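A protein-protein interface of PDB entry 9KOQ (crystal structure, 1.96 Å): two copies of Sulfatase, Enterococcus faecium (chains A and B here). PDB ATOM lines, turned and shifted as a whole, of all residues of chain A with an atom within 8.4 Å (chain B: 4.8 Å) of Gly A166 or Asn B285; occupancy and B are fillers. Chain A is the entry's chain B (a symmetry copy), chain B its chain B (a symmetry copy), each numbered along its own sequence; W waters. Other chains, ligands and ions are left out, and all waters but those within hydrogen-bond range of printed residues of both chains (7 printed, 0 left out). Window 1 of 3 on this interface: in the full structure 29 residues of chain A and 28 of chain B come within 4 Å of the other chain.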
ATOM      1  N   ASP A 161      24.592  -0.428  15.754  1.00  0.00           N
ATOM      2  CA  ASP A 161      25.733  -0.586  14.851  1.00  0.00           C
ATOM      3  C   ASP A 161      25.246  -0.516  13.408  1.00  0.00           C
ATOM      4  O   ASP A 161      24.043  -0.592  13.124  1.00  0.00           O
ATOM      5  CB  ASP A 161      26.480  -1.913  15.091  1.00  0.00           C
ATOM      6  CG  ASP A 161      27.963  -1.878  14.629  1.00  0.00           C
ATOM      7  OD1 ASP A 161      28.426  -0.895  13.992  1.00  0.00           O
ATOM      8  OD2 ASP A 161      28.670  -2.882  14.870  1.00  0.00           O
ATOM      9  N   LEU A 162      26.214  -0.409  12.491  1.00  0.00           N
ATOM     10  CA  LEU A 162      25.938  -0.252  11.063  1.00  0.00           C
ATOM     11  C   LEU A 162      25.348  -1.496  10.402  1.00  0.00           C
ATOM     12  O   LEU A 162      24.763  -1.371   9.321  1.00  0.00           O
ATOM     13  CB  LEU A 162      27.223   0.115  10.308  1.00  0.00           C
ATOM     14  CG  LEU A 162      27.917   1.438  10.575  1.00  0.00           C
ATOM     15  CD1 LEU A 162      28.991   1.662   9.516  1.00  0.00           C
ATOM     16  CD2 LEU A 162      26.879   2.573  10.565  1.00  0.00           C
ATOM     17  N   ILE A 163      25.516  -2.687  10.980  1.00  0.00           N
ATOM     18  CA  ILE A 163      25.105  -3.930  10.315  1.00  0.00           C
ATOM     19  C   ILE A 163      23.860  -4.546  10.960  1.00  0.00           C
ATOM     20  O   ILE A 163      23.626  -5.749  10.804  1.00  0.00           O
ATOM     21  CB  ILE A 163      26.236  -4.977  10.288  1.00  0.00           C
ATOM     22  CG1 ILE A 163      26.601  -5.425  11.713  1.00  0.00           C
ATOM     23  CG2 ILE A 163      27.442  -4.459   9.545  1.00  0.00           C
ATOM     24  CD1 ILE A 163      27.949  -6.090  11.839  1.00  0.00           C
ATOM     25  N   ASP A 164      23.052  -3.758  11.677  1.00  0.00           N
ATOM     26  CA  ASP A 164      22.037  -4.363  12.536  1.00  0.00           C
ATOM     27  C   ASP A 164      20.964  -5.109  11.743  1.00  0.00           C
ATOM     28  O   ASP A 164      20.403  -6.086  12.250  1.00  0.00           O
ATOM     29  CB  ASP A 164      21.381  -3.306  13.430  1.00  0.00           C
ATOM     30  CG  ASP A 164      22.312  -2.825  14.541  1.00  0.00           C
ATOM     31  OD1 ASP A 164      23.353  -3.479  14.757  1.00  0.00           O
ATOM     32  OD2 ASP A 164      21.999  -1.808  15.208  1.00  0.00           O
ATOM     33  N   ASP A 165      20.657  -4.689  10.516  1.00  0.00           N
ATOM     34  CA  ASP A 165      19.600  -5.366   9.764  1.00  0.00           C
ATOM     35  C   ASP A 165      20.103  -6.533   8.911  1.00  0.00           C
ATOM     36  O   ASP A 165      19.292  -7.191   8.241  1.00  0.00           O
ATOM     37  CB  ASP A 165      18.827  -4.358   8.892  1.00  0.00           C
ATOM     38  CG  ASP A 165      19.686  -3.722   7.797  1.00  0.00           C
ATOM     39  OD1 ASP A 165      20.782  -4.248   7.490  1.00  0.00           O
ATOM     40  OD2 ASP A 165      19.250  -2.684   7.239  1.00  0.00           O
ATOM     41  N   GLY A 166      21.408  -6.803   8.919  1.00  0.00           N
ATOM     42  CA  GLY A 166      21.958  -7.958   8.245  1.00  0.00           C
ATOM     43  C   GLY A 166      22.367  -7.767   6.804  1.00  0.00           C
ATOM     44  O   GLY A 166      22.742  -8.754   6.154  1.00  0.00           O
ATOM     45  N   LEU A 167      22.321  -6.541   6.279  1.00  0.00           N
ATOM     46  CA  LEU A 167      22.684  -6.300   4.889  1.00  0.00           C
ATOM     47  C   LEU A 167      24.176  -6.002   4.766  1.00  0.00           C
ATOM     48  O   LEU A 167      24.729  -5.210   5.540  1.00  0.00           O
ATOM     49  CB  LEU A 167      21.870  -5.142   4.305  1.00  0.00           C
ATOM     50  CG  LEU A 167      20.363  -5.347   4.126  1.00  0.00           C
ATOM     51  CD1 LEU A 167      19.709  -4.052   3.604  1.00  0.00           C
ATOM     52  CD2 LEU A 167      20.076  -6.509   3.201  1.00  0.00           C
ATOM     53  N   ASN A 168      24.811  -6.625   3.766  1.00  0.00           N
ATOM     54  CA  ASN A 168      26.239  -6.477   3.482  1.00  0.00           C
ATOM     55  C   ASN A 168      26.482  -5.326   2.501  1.00  0.00           C
ATOM     56  O   ASN A 168      25.685  -5.086   1.588  1.00  0.00           O
ATOM     57  CB  ASN A 168      26.786  -7.791   2.909  1.00  0.00           C
ATOM     58  CG  ASN A 168      28.292  -7.885   2.973  1.00  0.00           C
ATOM     59  OD1 ASN A 168      29.000  -7.041   2.419  1.00  0.00           O
ATOM     60  ND2 ASN A 168      28.795  -8.940   3.622  1.00  0.00           N
ATOM     61  N   CYS A 169      27.609  -4.624   2.676  1.00  0.00           N
ATOM     62  CA  CYS A 169      27.857  -3.444   1.844  1.00  0.00           C
ATOM     63  C   CYS A 169      28.240  -3.781   0.407  1.00  0.00           C
ATOM     64  O   CYS A 169      28.289  -2.871  -0.424  1.00  0.00           O
ATOM     65  CB  CYS A 169      28.946  -2.560   2.457  1.00  0.00           C
ATOM     66  SG  CYS A 169      30.579  -3.313   2.450  1.00  0.00           S
ATOM     67  N   ASN A 170      28.515  -5.044   0.081  1.00  0.00           N
ATOM     68  CA  ASN A 170      28.737  -5.431  -1.308  1.00  0.00           C
ATOM     69  C   ASN A 170      27.651  -6.364  -1.823  1.00  0.00           C
ATOM     70  O   ASN A 170      27.885  -7.114  -2.777  1.00  0.00           O
ATOM     71  CB  ASN A 170      30.107  -6.085  -1.490  1.00  0.00           C
ATOM     72  CG  ASN A 170      31.239  -5.121  -1.236  1.00  0.00           C
ATOM     73  OD1 ASN A 170      31.375  -4.125  -1.938  1.00  0.00           O
ATOM     74  ND2 ASN A 170      32.100  -5.451  -0.279  1.00  0.00           N
ATOM     75  N   SER A 171      26.464  -6.316  -1.227  1.00  0.00           N
ATOM     76  CA  SER A 171      25.408  -7.278  -1.490  1.00  0.00           C
ATOM     77  C   SER A 171      24.244  -6.648  -2.246  1.00  0.00           C
ATOM     78  O   SER A 171      23.914  -5.470  -2.045  1.00  0.00           O
ATOM     79  CB  SER A 171      24.907  -7.872  -0.174  1.00  0.00           C
ATOM     80  OG  SER A 171      23.911  -8.840  -0.410  1.00  0.00           O
ATOM     81  N   GLU A 173      21.294  -7.886  -1.722  1.00  0.00           N
ATOM     82  CA  GLU A 173      20.163  -7.994  -0.809  1.00  0.00           C
ATOM     83  C   GLU A 173      19.674  -6.597  -0.418  1.00  0.00           C
ATOM     84  O   GLU A 173      20.460  -5.653  -0.319  1.00  0.00           O
ATOM     85  CB  GLU A 173      20.578  -8.795   0.432  1.00  0.00           C
ATOM     86  CG  GLU A 173      20.603 -10.337   0.263  1.00  0.00           C
ATOM     87  CD  GLU A 173      21.218 -11.056   1.475  1.00  0.00           C
ATOM     88  OE1 GLU A 173      21.021 -10.589   2.619  1.00  0.00           O
ATOM     89  OE2 GLU A 173      21.848 -12.125   1.309  1.00  0.00           O
ATOM     90  N   ALA A 174      18.363  -6.456  -0.195  1.00  0.00           N
ATOM     91  CA  ALA A 174      17.797  -5.147   0.128  1.00  0.00           C
ATOM     92  C   ALA A 174      16.551  -5.282   0.989  1.00  0.00           C
ATOM     93  O   ALA A 174      15.822  -6.275   0.907  1.00  0.00           O
ATOM     94  CB  ALA A 174      17.445  -4.348  -1.127  1.00  0.00           C
ATOM     95  N   ARG A 175      16.300  -4.250   1.784  1.00  0.00           N
ATOM     96  CA  ARG A 175      15.147  -4.174   2.675  1.00  0.00           C
ATOM     97  C   ARG A 175      15.140  -2.778   3.302  1.00  0.00           C
ATOM     98  O   ARG A 175      16.165  -2.098   3.284  1.00  0.00           O
ATOM     99  CB  ARG A 175      15.202  -5.272   3.756  1.00  0.00           C
ATOM    100  CG  ARG A 175      16.342  -5.110   4.762  1.00  0.00           C
ATOM    101  CD  ARG A 175      15.918  -5.633   6.127  1.00  0.00           C
ATOM    102  NE  ARG A 175      15.054  -4.650   6.772  1.00  0.00           N
ATOM    103  CZ  ARG A 175      14.374  -4.858   7.889  1.00  0.00           C
ATOM    104  NH1 ARG A 175      14.365  -6.046   8.486  1.00  0.00           N
ATOM    105  NH2 ARG A 175      13.679  -3.852   8.418  1.00  0.00           N
ATOM    106  N   MET A 178      15.733  -0.114   9.254  1.00  0.00           N
ATOM    107  CA  MET A 178      14.987  -0.771  10.326  1.00  0.00           C
ATOM    108  C   MET A 178      14.712   0.140  11.525  1.00  0.00           C
ATOM    109  O   MET A 178      13.944  -0.247  12.418  1.00  0.00           O
ATOM    110  CB  MET A 178      15.730  -2.029  10.796  1.00  0.00           C
ATOM    111  CG  MET A 178      16.878  -1.770  11.761  1.00  0.00           C
ATOM    112  SD  MET A 178      17.671  -3.311  12.340  1.00  0.00           S
ATOM    113  CE  MET A 178      16.638  -3.717  13.753  1.00  0.00           C
ATOM    114  N   PRO A 218      24.917  -0.990   2.128  1.00  0.00           N
ATOM    115  CA  PRO A 218      23.619  -1.678   2.208  1.00  0.00           C
ATOM    116  C   PRO A 218      22.447  -0.906   1.599  1.00  0.00           C
ATOM    117  O   PRO A 218      22.337   0.317   1.692  1.00  0.00           O
ATOM    118  CB  PRO A 218      23.422  -1.899   3.711  1.00  0.00           C
ATOM    119  CG  PRO A 218      24.465  -1.095   4.383  1.00  0.00           C
ATOM    120  CD  PRO A 218      25.591  -0.963   3.439  1.00  0.00           C
ATOM    121  N   ASN A 220      19.330  -0.014   2.041  1.00  0.00           N
ATOM    122  CA  ASN A 220      18.307   0.165   3.075  1.00  0.00           C
ATOM    123  C   ASN A 220      17.817   1.609   3.124  1.00  0.00           C
ATOM    124  O   ASN A 220      18.088   2.348   4.083  1.00  0.00           O
ATOM    125  CB  ASN A 220      18.821  -0.311   4.440  1.00  0.00           C
ATOM    126  CG  ASN A 220      20.216   0.210   4.784  1.00  0.00           C
ATOM    127  OD1 ASN A 220      20.738   1.133   4.162  1.00  0.00           O
ATOM    128  ND2 ASN A 220      20.819  -0.388   5.803  1.00  0.00           N
ATOM    129  N   ASP A 253      26.311 -15.914  -4.837  1.00  0.00           N
ATOM    130  CA  ASP A 253      26.902 -15.420  -3.596  1.00  0.00           C
ATOM    131  C   ASP A 253      26.161 -14.157  -3.161  1.00  0.00           C
ATOM    132  O   ASP A 253      25.742 -13.352  -4.001  1.00  0.00           O
ATOM    133  CB  ASP A 253      28.394 -15.107  -3.824  1.00  0.00           C
ATOM    134  CG  ASP A 253      29.180 -14.886  -2.517  1.00  0.00           C
ATOM    135  OD1 ASP A 253      29.008 -13.829  -1.861  1.00  0.00           O
ATOM    136  OD2 ASP A 253      30.039 -15.736  -2.183  1.00  0.00           O
ATOM    137  N   VAL A 254      25.983 -13.979  -1.846  1.00  0.00           N
ATOM    138  CA  VAL A 254      25.288 -12.768  -1.409  1.00  0.00           C
ATOM    139  C   VAL A 254      26.089 -11.506  -1.748  1.00  0.00           C
ATOM    140  O   VAL A 254      25.505 -10.425  -1.841  1.00  0.00           O
ATOM    141  CB  VAL A 254      24.924 -12.822   0.089  1.00  0.00           C
ATOM    142  CG1 VAL A 254      24.127 -14.089   0.397  1.00  0.00           C
ATOM    143  CG2 VAL A 254      26.156 -12.767   0.952  1.00  0.00           C
ATOM    144  N   CYS A 255      27.403 -11.616  -1.971  1.00  0.00           N
ATOM    145  CA  CYS A 255      28.229 -10.497  -2.420  1.00  0.00           C
ATOM    146  C   CYS A 255      28.778 -10.746  -3.826  1.00  0.00           C
ATOM    147  O   CYS A 255      29.901 -10.351  -4.153  1.00  0.00           O
ATOM    148  CB  CYS A 255      29.363 -10.242  -1.429  1.00  0.00           C
ATOM    149  SG  CYS A 255      28.770  -9.774   0.237  1.00  0.00           S
ATOM    150  N   THR B  36      20.943 -15.932   1.994  1.00  0.00           N
ATOM    151  CA  THR B  36      22.175 -16.238   2.723  1.00  0.00           C
ATOM    152  C   THR B  36      22.335 -17.739   2.947  1.00  0.00           C
ATOM    153  O   THR B  36      23.423 -18.296   2.751  1.00  0.00           O
ATOM    154  CB  THR B  36      22.192 -15.511   4.070  1.00  0.00           C
ATOM    155  OG1 THR B  36      21.959 -14.112   3.872  1.00  0.00           O
ATOM    156  CG2 THR B  36      23.520 -15.744   4.780  1.00  0.00           C
ATOM    157  N   ASP B 281      17.311 -15.516   8.122  1.00  0.00           N
ATOM    158  CA  ASP B 281      18.328 -15.527   7.075  1.00  0.00           C
ATOM    159  C   ASP B 281      19.149 -14.239   7.089  1.00  0.00           C
ATOM    160  O   ASP B 281      20.384 -14.284   7.070  1.00  0.00           O
ATOM    161  CB  ASP B 281      17.654 -15.751   5.720  1.00  0.00           C
ATOM    162  CG  ASP B 281      18.638 -15.727   4.565  1.00  0.00           C
ATOM    163  OD1 ASP B 281      18.938 -14.618   4.072  1.00  0.00           O
ATOM    164  OD2 ASP B 281      19.090 -16.816   4.141  1.00  0.00           O
ATOM    165  N   HIS B 282      18.477 -13.079   7.161  1.00  0.00           N
ATOM    166  CA  HIS B 282      19.197 -11.806   7.258  1.00  0.00           C
ATOM    167  C   HIS B 282      20.039 -11.747   8.527  1.00  0.00           C
ATOM    168  O   HIS B 282      21.192 -11.292   8.501  1.00  0.00           O
ATOM    169  CB  HIS B 282      18.213 -10.624   7.223  1.00  0.00           C
ATOM    170  CG  HIS B 282      17.806 -10.206   5.842  1.00  0.00           C
ATOM    171  ND1 HIS B 282      16.649  -9.498   5.588  1.00  0.00           N
ATOM    172  CD2 HIS B 282      18.415 -10.374   4.642  1.00  0.00           C
ATOM    173  CE1 HIS B 282      16.548  -9.270   4.289  1.00  0.00           C
ATOM    174  NE2 HIS B 282      17.608  -9.791   3.691  1.00  0.00           N
ATOM    175  N   GLN B 283      19.487 -12.212   9.652  1.00  0.00           N
ATOM    176  CA  GLN B 283      20.237 -12.115  10.903  1.00  0.00           C
ATOM    177  C   GLN B 283      21.447 -13.049  10.916  1.00  0.00           C
ATOM    178  O   GLN B 283      22.490 -12.711  11.495  1.00  0.00           O
ATOM    179  CB  GLN B 283      19.292 -12.364  12.088  1.00  0.00           C
ATOM    180  CG  GLN B 283      18.326 -11.175  12.308  1.00  0.00           C
ATOM    181  CD  GLN B 283      19.079  -9.907  12.704  1.00  0.00           C
ATOM    182  OE1 GLN B 283      19.822  -9.904  13.683  1.00  0.00           O
ATOM    183  NE2 GLN B 283      18.889  -8.830  11.942  1.00  0.00           N
ATOM    184  N   ILE B 284      21.354 -14.205  10.261  1.00  0.00           N
ATOM    185  CA  ILE B 284      22.541 -15.048  10.115  1.00  0.00           C
ATOM    186  C   ILE B 284      23.603 -14.343   9.275  1.00  0.00           C
ATOM    187  O   ILE B 284      24.807 -14.440   9.558  1.00  0.00           O
ATOM    188  CB  ILE B 284      22.161 -16.429   9.542  1.00  0.00           C
ATOM    189  CG1 ILE B 284      21.515 -17.276  10.645  1.00  0.00           C
ATOM    190  CG2 ILE B 284      23.378 -17.129   8.938  1.00  0.00           C
ATOM    191  CD1 ILE B 284      20.831 -18.584  10.143  1.00  0.00           C
ATOM    192  N   ASN B 285      23.178 -13.599   8.260  1.00  0.00           N
ATOM    193  CA  ASN B 285      24.135 -12.831   7.473  1.00  0.00           C
ATOM    194  C   ASN B 285      24.830 -11.779   8.331  1.00  0.00           C
ATOM    195  O   ASN B 285      26.036 -11.546   8.188  1.00  0.00           O
ATOM    196  CB  ASN B 285      23.444 -12.179   6.287  1.00  0.00           C
ATOM    197  CG  ASN B 285      24.428 -11.786   5.222  1.00  0.00           C
ATOM    198  OD1 ASN B 285      25.178 -12.629   4.731  1.00  0.00           O
ATOM    199  ND2 ASN B 285      24.464 -10.507   4.885  1.00  0.00           N
ATOM    200  N   ARG B 286      24.083 -11.149   9.242  1.00  0.00           N
ATOM    201  CA  ARG B 286      24.680 -10.253  10.229  1.00  0.00           C
ATOM    202  C   ARG B 286      25.781 -10.954  11.015  1.00  0.00           C
ATOM    203  O   ARG B 286      26.866 -10.400  11.220  1.00  0.00           O
ATOM    204  CB  ARG B 286      23.581  -9.740  11.166  1.00  0.00           C
ATOM    205  CG  ARG B 286      24.035  -8.833  12.283  1.00  0.00           C
ATOM    206  CD  ARG B 286      22.809  -8.393  13.118  1.00  0.00           C
ATOM    207  NE  ARG B 286      23.246  -7.733  14.344  1.00  0.00           N
ATOM    208  CZ  ARG B 286      22.635  -7.846  15.515  1.00  0.00           C
ATOM    209  NH1 ARG B 286      21.532  -8.574  15.657  1.00  0.00           N
ATOM    210  NH2 ARG B 286      23.158  -7.239  16.576  1.00  0.00           N
ATOM    211  N   PHE B 287      25.515 -12.182  11.470  1.00  0.00           N
ATOM    212  CA  PHE B 287      26.517 -12.906  12.239  1.00  0.00           C
ATOM    213  C   PHE B 287      27.732 -13.254  11.384  1.00  0.00           C
ATOM    214  O   PHE B 287      28.869 -13.222  11.868  1.00  0.00           O
ATOM    215  CB  PHE B 287      25.915 -14.182  12.846  1.00  0.00           C
ATOM    216  CG  PHE B 287      26.889 -14.942  13.691  1.00  0.00           C
ATOM    217  CD1 PHE B 287      27.157 -14.523  14.989  1.00  0.00           C
ATOM    218  CD2 PHE B 287      27.572 -16.042  13.187  1.00  0.00           C
ATOM    219  CE1 PHE B 287      28.090 -15.199  15.781  1.00  0.00           C
ATOM    220  CE2 PHE B 287      28.481 -16.718  13.970  1.00  0.00           C
ATOM    221  CZ  PHE B 287      28.741 -16.297  15.269  1.00  0.00           C
ATOM    222  N   LEU B 288      27.513 -13.593  10.110  1.00  0.00           N
ATOM    223  CA  LEU B 288      28.636 -13.852   9.217  1.00  0.00           C
ATOM    224  C   LEU B 288      29.510 -12.612   9.058  1.00  0.00           C
ATOM    225  O   LEU B 288      30.740 -12.707   9.081  1.00  0.00           O
ATOM    226  CB  LEU B 288      28.127 -14.324   7.857  1.00  0.00           C
ATOM    227  CG  LEU B 288      27.370 -15.658   7.766  1.00  0.00           C
ATOM    228  CD1 LEU B 288      27.056 -15.956   6.307  1.00  0.00           C
ATOM    229  CD2 LEU B 288      28.185 -16.784   8.387  1.00  0.00           C
ATOM    230  N   MET B 289      28.892 -11.440   8.895  1.00  0.00           N
ATOM    231  CA  MET B 289      29.660 -10.204   8.785  1.00  0.00           C
ATOM    232  C   MET B 289      30.494  -9.978  10.043  1.00  0.00           C
ATOM    233  O   MET B 289      31.664  -9.588   9.963  1.00  0.00           O
ATOM    234  CB  MET B 289      28.698  -9.048   8.548  1.00  0.00           C
ATOM    235  CG  MET B 289      28.175  -9.034   7.118  1.00  0.00           C
ATOM    236  SD  MET B 289      27.301  -7.521   6.655  1.00  0.00           S
ATOM    237  CE  MET B 289      25.776  -7.705   7.575  1.00  0.00           C
HETATM  238  O   HOH W   1      27.792 -11.566   4.338  1.00  0.00           O
HETATM  239  O   HOH W   2      29.338  -5.156   4.947  1.00  0.00           O
HETATM  240  O   HOH W   3      19.537  -6.006  15.042  1.00  0.00           O
HETATM  241  O   HOH W   4      25.188  -5.766  14.833  1.00  0.00           O
HETATM  242  O   HOH W   5      17.010  -8.210   9.491  1.00  0.00           O
HETATM  243  O   HOH W   6      23.586  -8.789   2.371  1.00  0.00           O
HETATM  244  O   HOH W   7      23.844  -3.890  17.192  1.00  0.00           O
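O of Asp A164 sits at hydrogen-bond distance from NE2 of Gln B283, 3.1 Å away.
O of Gly A166 is in hydrogen-bond range of ND2 of Asn B285, at 2.8 Å.
ND2 of Asn A168 sits close to SD of Met B289 (3.7 Å).
The side-chain hydroxyl (OG1) of Thr B36 sits at hydrogen-bond distance from the side-chain carboxylate (OE2) of Glu A173 (3.2 Å).
The backbone carbonyl oxygen of Leu A167 sits close to the side-chain sulfur of Met B289, at 3.6 Å.
The backbone NH (N) of Asp A161 sits at hydrogen-bond distance from the side-chain carboxylate (OD2) of Asp A164, 3.0 Å away.
The side-chain carboxylate of Asp A165 sits at hydrogen-bond distance from the side-chain amide nitrogen of Asn A220 (3.1 Å).
The side-chain amide oxygen of Asn A168 lies within hydrogen-bond range of the backbone NH of Asn A170, at 3.1 Å.
The side-chain amide nitrogen of Asn A168 lies close to the side-chain sulfur of Cys A255, 3.5 Å away.
The side-chain hydroxyl (OG) of Ser A171 sits at hydrogen-bond distance from the backbone NH (N) of Glu A173, at 3.1 Å.
OD2 of Asp B281 sits at hydrogen-bond distance from N of Thr B36 (3.0 Å).
Ile A163 touches Met B289 (CB to CE, 3.9 Å).
O of Asp A164 touches CD of Arg B286 (3.4 Å).
His B282 touches Asp A165 (CB to O, 3.7 Å).
Asp A165 touches Gln B283 (C to NE2, 3.99 Å).
Gly A166 touches His B282.
Arg B286 touches Gly A166 (CB to CA, 3.8 Å).
C of Gly A166 touches CE of Met B289, at 3.5 Å.
His B282 touches Arg A175.
CA of Thr B36 touches CG1 of Val A254 (3.7 Å).
Val A254 touches Asn B285 (CG2 to OD1, 3.9 Å).
Of chain B, only His B282 (3.4 Å), Asn B285 (2.8 Å), Arg B286 (3.8 Å) and Met B289 (3.5 Å) come within 4 Å of Gly A166.
Ala A174 touches none of the printed residues of chain B.
Of the printed residues of chain A, Thr B36 touches Glu A173 (3.2 Å) and Val A254 (3.7 Å).
Printed residues of chain A within 4 Å of Gln B283: Asp A164 (3.1 Å) and Asp A165 (3.99 Å).
Asn B285 touches just these residues of chain A: Gly A166 and Val A254.
Printed residues of chain A within 4 Å of Met B289: Ile A163, Gly A166, Leu A167 and Asn A168.
The nearest residue of chain B that does not touch Gly A166 is Gln B283 (4.4 Å).
The nearest residue of chain A that does not touch Asn B285 is Asn A168 (4.1 Å).
The nearest printed residue of chain B that does not touch Asp A165 is Arg B286 (5.0 Å).
No position is printed for both chains.
Water W7 lies within hydrogen-bond range of the side-chain carboxylate (OD1) of Asp A164 (2.5 Å) and the guanidinium group (NH2) of Arg B286 (3.5 Å).
Water W5 lies within hydrogen-bond range of O of Asp A165 (2.8 Å) and NE2 of Gln B283 (3.1 Å).
Water W6 lies within hydrogen-bond range of the side-chain hydroxyl of Ser A171 (2.8 Å), the backbone NH of Asn A168 (2.9 Å), the side-chain carboxylate of Glu A173 (3.1 Å) and the side-chain amide nitrogen of Asn B285 (3.2 Å).
Water W4 bridges the guanidinium group (NE) of Arg B286 (2.8 Å) and the side-chain carboxylate (OD1) of Asp A164 (2.9 Å).
Water W2 lies within hydrogen-bond range of the backbone NH of Cys A169 (2.9 Å), the side-chain amide oxygen of Asn A168 (3.2 Å) and the side-chain sulfur of Met B289 (3.6 Å).
Water W3 lies within hydrogen-bond range of the backbone carbonyl oxygen (O) of Asp A164 (2.9 Å) and the guanidinium group (NH1) of Arg B286 (3.3 Å).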
